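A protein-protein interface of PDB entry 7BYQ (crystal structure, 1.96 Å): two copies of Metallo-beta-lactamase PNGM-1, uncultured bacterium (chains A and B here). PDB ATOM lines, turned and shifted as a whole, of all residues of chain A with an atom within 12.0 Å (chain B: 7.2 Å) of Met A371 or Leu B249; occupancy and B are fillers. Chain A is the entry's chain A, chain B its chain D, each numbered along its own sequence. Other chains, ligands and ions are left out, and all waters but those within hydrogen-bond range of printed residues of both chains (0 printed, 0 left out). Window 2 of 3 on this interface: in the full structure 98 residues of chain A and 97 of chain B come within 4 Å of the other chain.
NH1 of Arg A356 lies within hydrogen-bond range of O of Asp B254, 2.7 Å away.
OD1 of Asn A363 sits at hydrogen-bond distance from NE1 of Trp A366 (3.2 Å).
The backbone carbonyl oxygen (O) of Ala B248 is in hydrogen-bond range of the side-chain hydroxyl (OG) of Ser B234 (2.6 Å).
The backbone carbonyl oxygen (O) of Val A359 sits at hydrogen-bond distance from the side-chain amide nitrogen (ND2) of Asn A363, at 2.4 Å.
The backbone NH (N) of Ser B234 lies close to the side-chain amide nitrogen (ND2) of Asn B252 (3.5 Å).
Among the printed residues, merely in contact across the chains: Phe A370 with Asp B235 (3.2 Å), Trp A366 with Ser B234 (3.2 Å), Phe A370 with Leu B249 (3.3 Å), Phe A370 with Ser B234 (3.4 Å), Met A371 with Leu B249 (3.5 Å), Trp A366 with Leu B253 (3.6 Å), Lys A367 with Leu B253 (3.6 Å), Asn A363 with Leu B253 (3.7 Å), Phe A370 with Met B238 (3.7 Å) and Phe A370 with Ala B245 (3.9 Å).
Printed residues of chain A within 4 Å of Leu B249: Phe A370 (3.3 Å) and Met A371 (3.5 Å).
Ser B234 touches just these residues of chain A: Trp A366 (3.2 Å) and Phe A370 (3.4 Å).
Of chain A, only Phe A370 comes within 4 Å of Ala B245.
No residue of chain A comes within 4 Å of Ala B248.
No residue of chain A comes within 4 Å of Arg B250.
No residue of chain A comes within 4 Å of Ile B251.
No residue of chain A comes within 4 Å of Asn B252.
Printed residues of chain A within 4 Å of Asp B235: Phe A370 (3.2 Å).
Of the printed residues of chain B, Trp A366 touches Ser B234 (3.2 Å) and Leu B253 (3.6 Å).
Of the printed residues of chain A, Met B238 touches Phe A370.
Of the printed residues of chain B, Asn A363 touches Leu B253.
His A365 touches none of the printed residues of chain B.
Glu A361 touches none of the printed residues of chain B.
Of the 15 printed residues of chain A, 6 touch a printed residue of chain B.
Printed residues of chain A that touch a printed residue of chain B: Arg A356, Asn A363, Trp A366, Lys A367, Phe A370 and Met A371.
Hydrophobic or aromatic side chains of chain B that line the printed part of chain A: Met B238, Leu B249 and Leu B253.
Among the printed residues, 11 pairs touch across the chains.
Among the printed residues, no Asp or Glu carboxylate lies within 4 Å of a Lys or Arg side-chain nitrogen of the other chain.
No position is printed for both chains.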
ATOM      1  N   ARG A 356      26.850 -32.067 -13.133  1.00  0.00           N
ATOM      2  CA  ARG A 356      26.044 -31.041 -12.412  1.00  0.00           C
ATOM      3  C   ARG A 356      24.587 -31.508 -12.312  1.00  0.00           C
ATOM      4  O   ARG A 356      24.130 -32.219 -13.221  1.00  0.00           O
ATOM      5  CB  ARG A 356      26.089 -29.686 -13.128  1.00  0.00           C
ATOM      6  CG  ARG A 356      27.355 -28.881 -12.889  1.00  0.00           C
ATOM      7  CD  ARG A 356      27.198 -27.453 -13.369  1.00  0.00           C
ATOM      8  NE  ARG A 356      28.420 -26.675 -13.228  1.00  0.00           N
ATOM      9  CZ  ARG A 356      28.875 -26.156 -12.087  1.00  0.00           C
ATOM     10  NH1 ARG A 356      28.224 -26.337 -10.949  1.00  0.00           N
ATOM     11  NH2 ARG A 356      29.997 -25.459 -12.088  1.00  0.00           N
ATOM     12  N   VAL A 359      19.083 -27.794 -10.243  1.00  0.00           N
ATOM     13  CA  VAL A 359      18.604 -27.308  -8.914  1.00  0.00           C
ATOM     14  C   VAL A 359      17.838 -25.990  -9.126  1.00  0.00           C
ATOM     15  O   VAL A 359      17.919 -25.106  -8.251  1.00  0.00           O
ATOM     16  CB  VAL A 359      19.783 -27.169  -7.923  1.00  0.00           C
ATOM     17  CG1 VAL A 359      20.365 -28.520  -7.536  1.00  0.00           C
ATOM     18  CG2 VAL A 359      20.883 -26.256  -8.444  1.00  0.00           C
ATOM     19  N   ASP A 360      17.102 -25.882 -10.242  1.00  0.00           N
ATOM     20  CA  ASP A 360      16.313 -24.682 -10.639  1.00  0.00           C
ATOM     21  C   ASP A 360      15.052 -24.562  -9.773  1.00  0.00           C
ATOM     22  O   ASP A 360      14.620 -23.417  -9.543  1.00  0.00           O
ATOM     23  CB  ASP A 360      15.912 -24.710 -12.122  1.00  0.00           C
ATOM     24  CG  ASP A 360      16.771 -23.854 -13.045  1.00  0.00           C
ATOM     25  OD1 ASP A 360      17.014 -22.676 -12.704  1.00  0.00           O
ATOM     26  OD2 ASP A 360      17.180 -24.370 -14.110  1.00  0.00           O
ATOM     27  N   GLU A 361      14.479 -25.685  -9.323  1.00  0.00           N
ATOM     28  CA  GLU A 361      13.156 -25.709  -8.639  1.00  0.00           C
ATOM     29  C   GLU A 361      13.353 -25.264  -7.187  1.00  0.00           C
ATOM     30  O   GLU A 361      12.794 -24.215  -6.812  1.00  0.00           O
ATOM     31  CB  GLU A 361      12.468 -27.083  -8.658  1.00  0.00           C
ATOM     32  CG  GLU A 361      12.948 -28.051  -9.731  1.00  0.00           C
ATOM     33  CD  GLU A 361      13.965 -29.075  -9.252  1.00  0.00           C
ATOM     34  OE1 GLU A 361      14.937 -29.347 -10.003  1.00  0.00           O
ATOM     35  OE2 GLU A 361      13.781 -29.611  -8.132  1.00  0.00           O
ATOM     36  N   ALA A 362      14.143 -26.035  -6.428  1.00  0.00           N
ATOM     37  CA  ALA A 362      14.307 -25.950  -4.953  1.00  0.00           C
ATOM     38  C   ALA A 362      14.887 -24.591  -4.533  1.00  0.00           C
ATOM     39  O   ALA A 362      14.602 -24.164  -3.395  1.00  0.00           O
ATOM     40  CB  ALA A 362      15.175 -27.090  -4.475  1.00  0.00           C
ATOM     41  N   ASN A 363      15.653 -23.940  -5.416  1.00  0.00           N
ATOM     42  CA  ASN A 363      16.310 -22.625  -5.177  1.00  0.00           C
ATOM     43  C   ASN A 363      15.381 -21.475  -5.592  1.00  0.00           C
ATOM     44  O   ASN A 363      15.538 -20.367  -5.030  1.00  0.00           O
ATOM     45  CB  ASN A 363      17.634 -22.507  -5.933  1.00  0.00           C
ATOM     46  CG  ASN A 363      18.640 -23.549  -5.496  1.00  0.00           C
ATOM     47  OD1 ASN A 363      19.577 -23.254  -4.757  1.00  0.00           O
ATOM     48  ND2 ASN A 363      18.422 -24.783  -5.914  1.00  0.00           N
ATOM     49  N   ALA A 364      14.471 -21.728  -6.544  1.00  0.00           N
ATOM     50  CA  ALA A 364      13.587 -20.723  -7.182  1.00  0.00           C
ATOM     51  C   ALA A 364      13.173 -19.645  -6.171  1.00  0.00           C
ATOM     52  O   ALA A 364      13.367 -18.461  -6.486  1.00  0.00           O
ATOM     53  CB  ALA A 364      12.377 -21.389  -7.796  1.00  0.00           C
ATOM     54  N   HIS A 365      12.650 -20.039  -5.002  1.00  0.00           N
ATOM     55  CA  HIS A 365      11.965 -19.140  -4.027  1.00  0.00           C
ATOM     56  C   HIS A 365      12.922 -18.108  -3.416  1.00  0.00           C
ATOM     57  O   HIS A 365      12.503 -16.930  -3.254  1.00  0.00           O
ATOM     58  CB  HIS A 365      11.280 -19.936  -2.915  1.00  0.00           C
ATOM     59  CG  HIS A 365      10.376 -19.075  -2.104  1.00  0.00           C
ATOM     60  ND1 HIS A 365      10.829 -18.340  -1.028  1.00  0.00           N
ATOM     61  CD2 HIS A 365       9.070 -18.768  -2.259  1.00  0.00           C
ATOM     62  CE1 HIS A 365       9.826 -17.646  -0.526  1.00  0.00           C
ATOM     63  NE2 HIS A 365       8.737 -17.893  -1.266  1.00  0.00           N
ATOM     64  N   TRP A 366      14.131 -18.536  -3.037  1.00  0.00           N
ATOM     65  CA  TRP A 366      15.196 -17.656  -2.485  1.00  0.00           C
ATOM     66  C   TRP A 366      15.899 -16.929  -3.636  1.00  0.00           C
ATOM     67  O   TRP A 366      16.528 -15.892  -3.379  1.00  0.00           O
ATOM     68  CB  TRP A 366      16.183 -18.460  -1.625  1.00  0.00           C
ATOM     69  CG  TRP A 366      17.330 -19.035  -2.398  1.00  0.00           C
ATOM     70  CD1 TRP A 366      17.475 -20.320  -2.827  1.00  0.00           C
ATOM     71  CD2 TRP A 366      18.489 -18.324  -2.867  1.00  0.00           C
ATOM     72  NE1 TRP A 366      18.652 -20.467  -3.508  1.00  0.00           N
ATOM     73  CE2 TRP A 366      19.292 -19.258  -3.555  1.00  0.00           C
ATOM     74  CE3 TRP A 366      18.933 -17.005  -2.754  1.00  0.00           C
ATOM     75  CZ2 TRP A 366      20.514 -18.906  -4.123  1.00  0.00           C
ATOM     76  CZ3 TRP A 366      20.133 -16.653  -3.329  1.00  0.00           C
ATOM     77  CH2 TRP A 366      20.914 -17.595  -3.997  1.00  0.00           C
ATOM     78  N   LYS A 367      15.794 -17.457  -4.859  1.00  0.00           N
ATOM     79  CA  LYS A 367      16.447 -16.894  -6.071  1.00  0.00           C
ATOM     80  C   LYS A 367      15.601 -15.735  -6.614  1.00  0.00           C
ATOM     81  O   LYS A 367      16.196 -14.715  -7.013  1.00  0.00           O
ATOM     82  CB  LYS A 367      16.651 -17.987  -7.124  1.00  0.00           C
ATOM     83  CG  LYS A 367      18.037 -18.022  -7.745  1.00  0.00           C
ATOM     84  CD  LYS A 367      18.284 -19.263  -8.565  1.00  0.00           C
ATOM     85  CE  LYS A 367      17.672 -19.192  -9.948  1.00  0.00           C
ATOM     86  NZ  LYS A 367      18.557 -18.474 -10.897  1.00  0.00           N
ATOM     87  N   GLN A 368      14.272 -15.895  -6.622  1.00  0.00           N
ATOM     88  CA  GLN A 368      13.295 -14.825  -6.965  1.00  0.00           C
ATOM     89  C   GLN A 368      13.480 -13.661  -5.986  1.00  0.00           C
ATOM     90  O   GLN A 368      13.844 -12.561  -6.448  1.00  0.00           O
ATOM     91  CB  GLN A 368      11.860 -15.367  -6.930  1.00  0.00           C
ATOM     92  CG  GLN A 368      10.791 -14.336  -7.276  1.00  0.00           C
ATOM     93  CD  GLN A 368       9.483 -14.961  -7.701  1.00  0.00           C
ATOM     94  OE1 GLN A 368       8.897 -14.581  -8.711  1.00  0.00           O
ATOM     95  NE2 GLN A 368       9.004 -15.928  -6.932  1.00  0.00           N
ATOM     96  N   GLU A 369      13.245 -13.909  -4.692  1.00  0.00           N
ATOM     97  CA  GLU A 369      13.285 -12.889  -3.600  1.00  0.00           C
ATOM     98  C   GLU A 369      14.634 -12.153  -3.659  1.00  0.00           C
ATOM     99  O   GLU A 369      14.631 -10.916  -3.880  1.00  0.00           O
ATOM    100  CB  GLU A 369      13.035 -13.558  -2.240  1.00  0.00           C
ATOM    101  CG  GLU A 369      12.278 -12.695  -1.233  1.00  0.00           C
ATOM    102  CD  GLU A 369      13.130 -11.851  -0.295  1.00  0.00           C
ATOM    103  OE1 GLU A 369      14.315 -12.211  -0.077  1.00  0.00           O
ATOM    104  OE2 GLU A 369      12.602 -10.836   0.233  1.00  0.00           O
ATOM    105  N   PHE A 370      15.744 -12.891  -3.531  1.00  0.00           N
ATOM    106  CA  PHE A 370      17.125 -12.339  -3.430  1.00  0.00           C
ATOM    107  C   PHE A 370      17.440 -11.417  -4.614  1.00  0.00           C
ATOM    108  O   PHE A 370      18.286 -10.512  -4.452  1.00  0.00           O
ATOM    109  CB  PHE A 370      18.179 -13.445  -3.358  1.00  0.00           C
ATOM    110  CG  PHE A 370      19.586 -12.934  -3.193  1.00  0.00           C
ATOM    111  CD1 PHE A 370      20.355 -12.597  -4.295  1.00  0.00           C
ATOM    112  CD2 PHE A 370      20.141 -12.776  -1.933  1.00  0.00           C
ATOM    113  CE1 PHE A 370      21.647 -12.122  -4.140  1.00  0.00           C
ATOM    114  CE2 PHE A 370      21.430 -12.293  -1.779  1.00  0.00           C
ATOM    115  CZ  PHE A 370      22.179 -11.962  -2.883  1.00  0.00           C
ATOM    116  N   MET A 371      16.796 -11.639  -5.762  1.00  0.00           N
ATOM    117  CA  MET A 371      16.965 -10.808  -6.983  1.00  0.00           C
ATOM    118  C   MET A 371      15.984  -9.627  -6.952  1.00  0.00           C
ATOM    119  O   MET A 371      15.552  -9.193  -8.042  1.00  0.00           O
ATOM    120  CB  MET A 371      16.773 -11.663  -8.241  1.00  0.00           C
ATOM    121  CG  MET A 371      18.073 -12.294  -8.718  1.00  0.00           C
ATOM    122  SD  MET A 371      17.901 -13.999  -9.305  1.00  0.00           S
ATOM    123  CE  MET A 371      18.842 -13.897 -10.826  1.00  0.00           C
ATOM    124  N   GLY A 372      15.684  -9.116  -5.748  1.00  0.00           N
ATOM    125  CA  GLY A 372      14.942  -7.863  -5.506  1.00  0.00           C
ATOM    126  C   GLY A 372      15.334  -7.220  -4.182  1.00  0.00           C
ATOM    127  O   GLY A 372      16.492  -7.163  -3.754  1.00  0.00           O
ATOM    128  N   SER B 234      23.537 -16.316   0.045  1.00  0.00           N
ATOM    129  CA  SER B 234      24.030 -15.213  -0.821  1.00  0.00           C
ATOM    130  C   SER B 234      23.911 -13.857  -0.109  1.00  0.00           C
ATOM    131  O   SER B 234      24.605 -12.929  -0.553  1.00  0.00           O
ATOM    132  CB  SER B 234      23.280 -15.184  -2.135  1.00  0.00           C
ATOM    133  OG  SER B 234      23.621 -16.292  -2.954  1.00  0.00           O
ATOM    134  N   ASP B 235      23.032 -13.736   0.902  1.00  0.00           N
ATOM    135  CA  ASP B 235      22.934 -12.558   1.811  1.00  0.00           C
ATOM    136  C   ASP B 235      24.209 -12.475   2.659  1.00  0.00           C
ATOM    137  O   ASP B 235      25.011 -11.537   2.449  1.00  0.00           O
ATOM    138  CB  ASP B 235      21.715 -12.634   2.740  1.00  0.00           C
ATOM    139  CG  ASP B 235      20.405 -12.168   2.123  1.00  0.00           C
ATOM    140  OD1 ASP B 235      19.910 -12.852   1.212  1.00  0.00           O
ATOM    141  OD2 ASP B 235      19.882 -11.124   2.576  1.00  0.00           O
ATOM    142  N   MET B 237      26.845 -13.516   2.354  1.00  0.00           N
ATOM    143  CA  MET B 237      28.034 -13.298   1.484  1.00  0.00           C
ATOM    144  C   MET B 237      28.221 -11.799   1.224  1.00  0.00           C
ATOM    145  O   MET B 237      29.385 -11.382   1.101  1.00  0.00           O
ATOM    146  CB  MET B 237      27.895 -14.042   0.152  1.00  0.00           C
ATOM    147  CG  MET B 237      27.847 -15.556   0.303  1.00  0.00           C
ATOM    148  SD  MET B 237      29.231 -16.217   1.278  1.00  0.00           S
ATOM    149  CE  MET B 237      30.611 -15.687   0.262  1.00  0.00           C
ATOM    150  N   MET B 238      27.121 -11.036   1.145  1.00  0.00           N
ATOM    151  CA  MET B 238      27.104  -9.560   0.927  1.00  0.00           C
ATOM    152  C   MET B 238      27.372  -8.811   2.240  1.00  0.00           C
ATOM    153  O   MET B 238      28.126  -7.818   2.198  1.00  0.00           O
ATOM    154  CB  MET B 238      25.755  -9.096   0.375  1.00  0.00           C
ATOM    155  CG  MET B 238      25.432  -9.664  -0.989  1.00  0.00           C
ATOM    156  SD  MET B 238      23.939  -8.925  -1.694  1.00  0.00           S
ATOM    157  CE  MET B 238      24.520  -7.268  -2.049  1.00  0.00           C
ATOM    158  N   GLN B 243      30.383  -8.590  -0.914  1.00  0.00           N
ATOM    159  CA  GLN B 243      30.263  -9.109  -2.303  1.00  0.00           C
ATOM    160  C   GLN B 243      29.169  -8.327  -3.026  1.00  0.00           C
ATOM    161  O   GLN B 243      28.149  -7.994  -2.426  1.00  0.00           O
ATOM    162  CB  GLN B 243      29.925 -10.603  -2.295  1.00  0.00           C
ATOM    163  CG  GLN B 243      30.951 -11.477  -1.582  1.00  0.00           C
ATOM    164  CD  GLN B 243      32.178 -11.749  -2.421  1.00  0.00           C
ATOM    165  OE1 GLN B 243      32.359 -12.841  -2.954  1.00  0.00           O
ATOM    166  NE2 GLN B 243      33.033 -10.747  -2.546  1.00  0.00           N
ATOM    167  N   PRO B 244      29.346  -7.989  -4.326  1.00  0.00           N
ATOM    168  CA  PRO B 244      28.225  -7.567  -5.164  1.00  0.00           C
ATOM    169  C   PRO B 244      27.239  -8.737  -5.293  1.00  0.00           C
ATOM    170  O   PRO B 244      27.694  -9.870  -5.278  1.00  0.00           O
ATOM    171  CB  PRO B 244      28.860  -7.203  -6.516  1.00  0.00           C
ATOM    172  CG  PRO B 244      30.340  -7.029  -6.215  1.00  0.00           C
ATOM    173  CD  PRO B 244      30.626  -7.950  -5.047  1.00  0.00           C
ATOM    174  N   ALA B 245      25.939  -8.444  -5.398  1.00  0.00           N
ATOM    175  CA  ALA B 245      24.845  -9.447  -5.364  1.00  0.00           C
ATOM    176  C   ALA B 245      25.105 -10.531  -6.418  1.00  0.00           C
ATOM    177  O   ALA B 245      24.980 -11.722  -6.078  1.00  0.00           O
ATOM    178  CB  ALA B 245      23.502  -8.783  -5.558  1.00  0.00           C
ATOM    179  N   GLN B 246      25.462 -10.117  -7.640  1.00  0.00           N
ATOM    180  CA  GLN B 246      25.817 -10.996  -8.795  1.00  0.00           C
ATOM    181  C   GLN B 246      26.720 -12.139  -8.312  1.00  0.00           C
ATOM    182  O   GLN B 246      26.283 -13.305  -8.383  1.00  0.00           O
ATOM    183  CB  GLN B 246      26.436 -10.135  -9.905  1.00  0.00           C
ATOM    184  CG  GLN B 246      27.423 -10.846 -10.824  1.00  0.00           C
ATOM    185  CD  GLN B 246      26.833 -11.989 -11.616  1.00  0.00           C
ATOM    186  OE1 GLN B 246      25.639 -12.273 -11.563  1.00  0.00           O
ATOM    187  NE2 GLN B 246      27.685 -12.658 -12.374  1.00  0.00           N
ATOM    188  N   LEU B 247      27.921 -11.815  -7.823  1.00  0.00           N
ATOM    189  CA  LEU B 247      28.914 -12.814  -7.340  1.00  0.00           C
ATOM    190  C   LEU B 247      28.321 -13.606  -6.168  1.00  0.00           C
ATOM    191  O   LEU B 247      28.416 -14.849  -6.202  1.00  0.00           O
ATOM    192  CB  LEU B 247      30.217 -12.111  -6.945  1.00  0.00           C
ATOM    193  CG  LEU B 247      31.289 -12.079  -8.035  1.00  0.00           C
ATOM    194  CD1 LEU B 247      30.854 -11.219  -9.214  1.00  0.00           C
ATOM    195  CD2 LEU B 247      32.615 -11.587  -7.482  1.00  0.00           C
ATOM    196  N   ALA B 248      27.728 -12.911  -5.188  1.00  0.00           N
ATOM    197  CA  ALA B 248      27.024 -13.506  -4.025  1.00  0.00           C
ATOM    198  C   ALA B 248      25.970 -14.511  -4.512  1.00  0.00           C
ATOM    199  O   ALA B 248      25.952 -15.645  -3.987  1.00  0.00           O
ATOM    200  CB  ALA B 248      26.401 -12.421  -3.180  1.00  0.00           C
ATOM    201  N   LEU B 249      25.135 -14.103  -5.476  1.00  0.00           N
ATOM    202  CA  LEU B 249      24.033 -14.911  -6.066  1.00  0.00           C
ATOM    203  C   LEU B 249      24.626 -16.177  -6.699  1.00  0.00           C
ATOM    204  O   LEU B 249      24.068 -17.266  -6.459  1.00  0.00           O
ATOM    205  CB  LEU B 249      23.285 -14.049  -7.094  1.00  0.00           C
ATOM    206  CG  LEU B 249      22.076 -14.687  -7.782  1.00  0.00           C
ATOM    207  CD1 LEU B 249      20.809 -14.493  -6.962  1.00  0.00           C
ATOM    208  CD2 LEU B 249      21.876 -14.117  -9.176  1.00  0.00           C
ATOM    209  N   ARG B 250      25.732 -16.038  -7.443  1.00  0.00           N
ATOM    210  CA  ARG B 250      26.361 -17.127  -8.243  1.00  0.00           C
ATOM    211  C   ARG B 250      27.058 -18.138  -7.322  1.00  0.00           C
ATOM    212  O   ARG B 250      26.875 -19.361  -7.546  1.00  0.00           O
ATOM    213  CB  ARG B 250      27.342 -16.546  -9.270  1.00  0.00           C
ATOM    214  CG  ARG B 250      26.670 -15.788 -10.407  1.00  0.00           C
ATOM    215  CD  ARG B 250      25.872 -16.702 -11.322  1.00  0.00           C
ATOM    216  NE  ARG B 250      24.543 -16.174 -11.623  1.00  0.00           N
ATOM    217  CZ  ARG B 250      23.471 -16.911 -11.908  1.00  0.00           C
ATOM    218  NH1 ARG B 250      23.544 -18.232 -11.929  1.00  0.00           N
ATOM    219  NH2 ARG B 250      22.316 -16.317 -12.165  1.00  0.00           N
ATOM    220  N   ILE B 251      27.818 -17.653  -6.331  1.00  0.00           N
ATOM    221  CA  ILE B 251      28.555 -18.488  -5.330  1.00  0.00           C
ATOM    222  C   ILE B 251      27.676 -19.682  -4.930  1.00  0.00           C
ATOM    223  O   ILE B 251      28.207 -20.810  -4.894  1.00  0.00           O
ATOM    224  CB  ILE B 251      29.012 -17.633  -4.123  1.00  0.00           C
ATOM    225  CG1 ILE B 251      30.267 -16.826  -4.473  1.00  0.00           C
ATOM    226  CG2 ILE B 251      29.235 -18.484  -2.877  1.00  0.00           C
ATOM    227  CD1 ILE B 251      30.651 -15.779  -3.459  1.00  0.00           C
ATOM    228  N   ASN B 252      26.373 -19.453  -4.718  1.00  0.00           N
ATOM    229  CA  ASN B 252      25.416 -20.431  -4.132  1.00  0.00           C
ATOM    230  C   ASN B 252      24.706 -21.270  -5.212  1.00  0.00           C
ATOM    231  O   ASN B 252      24.010 -22.231  -4.824  1.00  0.00           O
ATOM    232  CB  ASN B 252      24.402 -19.721  -3.227  1.00  0.00           C
ATOM    233  CG  ASN B 252      24.820 -19.709  -1.772  1.00  0.00           C
ATOM    234  OD1 ASN B 252      24.425 -20.585  -1.008  1.00  0.00           O
ATOM    235  ND2 ASN B 252      25.608 -18.722  -1.379  1.00  0.00           N
ATOM    236  N   LEU B 253      24.854 -20.946  -6.503  1.00  0.00           N
ATOM    237  CA  LEU B 253      24.226 -21.716  -7.618  1.00  0.00           C
ATOM    238  C   LEU B 253      25.282 -22.506  -8.405  1.00  0.00           C
ATOM    239  O   LEU B 253      24.994 -23.666  -8.778  1.00  0.00           O
ATOM    240  CB  LEU B 253      23.467 -20.762  -8.552  1.00  0.00           C
ATOM    241  CG  LEU B 253      21.970 -20.573  -8.286  1.00  0.00           C
ATOM    242  CD1 LEU B 253      21.336 -21.797  -7.632  1.00  0.00           C
ATOM    243  CD2 LEU B 253      21.721 -19.342  -7.434  1.00  0.00           C
ATOM    244  N   ASP B 254      26.438 -21.892  -8.668  1.00  0.00           N
ATOM    245  CA  ASP B 254      27.470 -22.396  -9.615  1.00  0.00           C
ATOM    246  C   ASP B 254      28.519 -23.219  -8.862  1.00  0.00           C
ATOM    247  O   ASP B 254      28.610 -24.431  -9.122  1.00  0.00           O
ATOM    248  CB  ASP B 254      28.113 -21.233 -10.376  1.00  0.00           C
ATOM    249  CG  ASP B 254      27.302 -20.752 -11.569  1.00  0.00           C
ATOM    250  OD1 ASP B 254      26.534 -21.563 -12.128  1.00  0.00           O
ATOM    251  OD2 ASP B 254      27.449 -19.571 -11.936  1.00  0.00           O
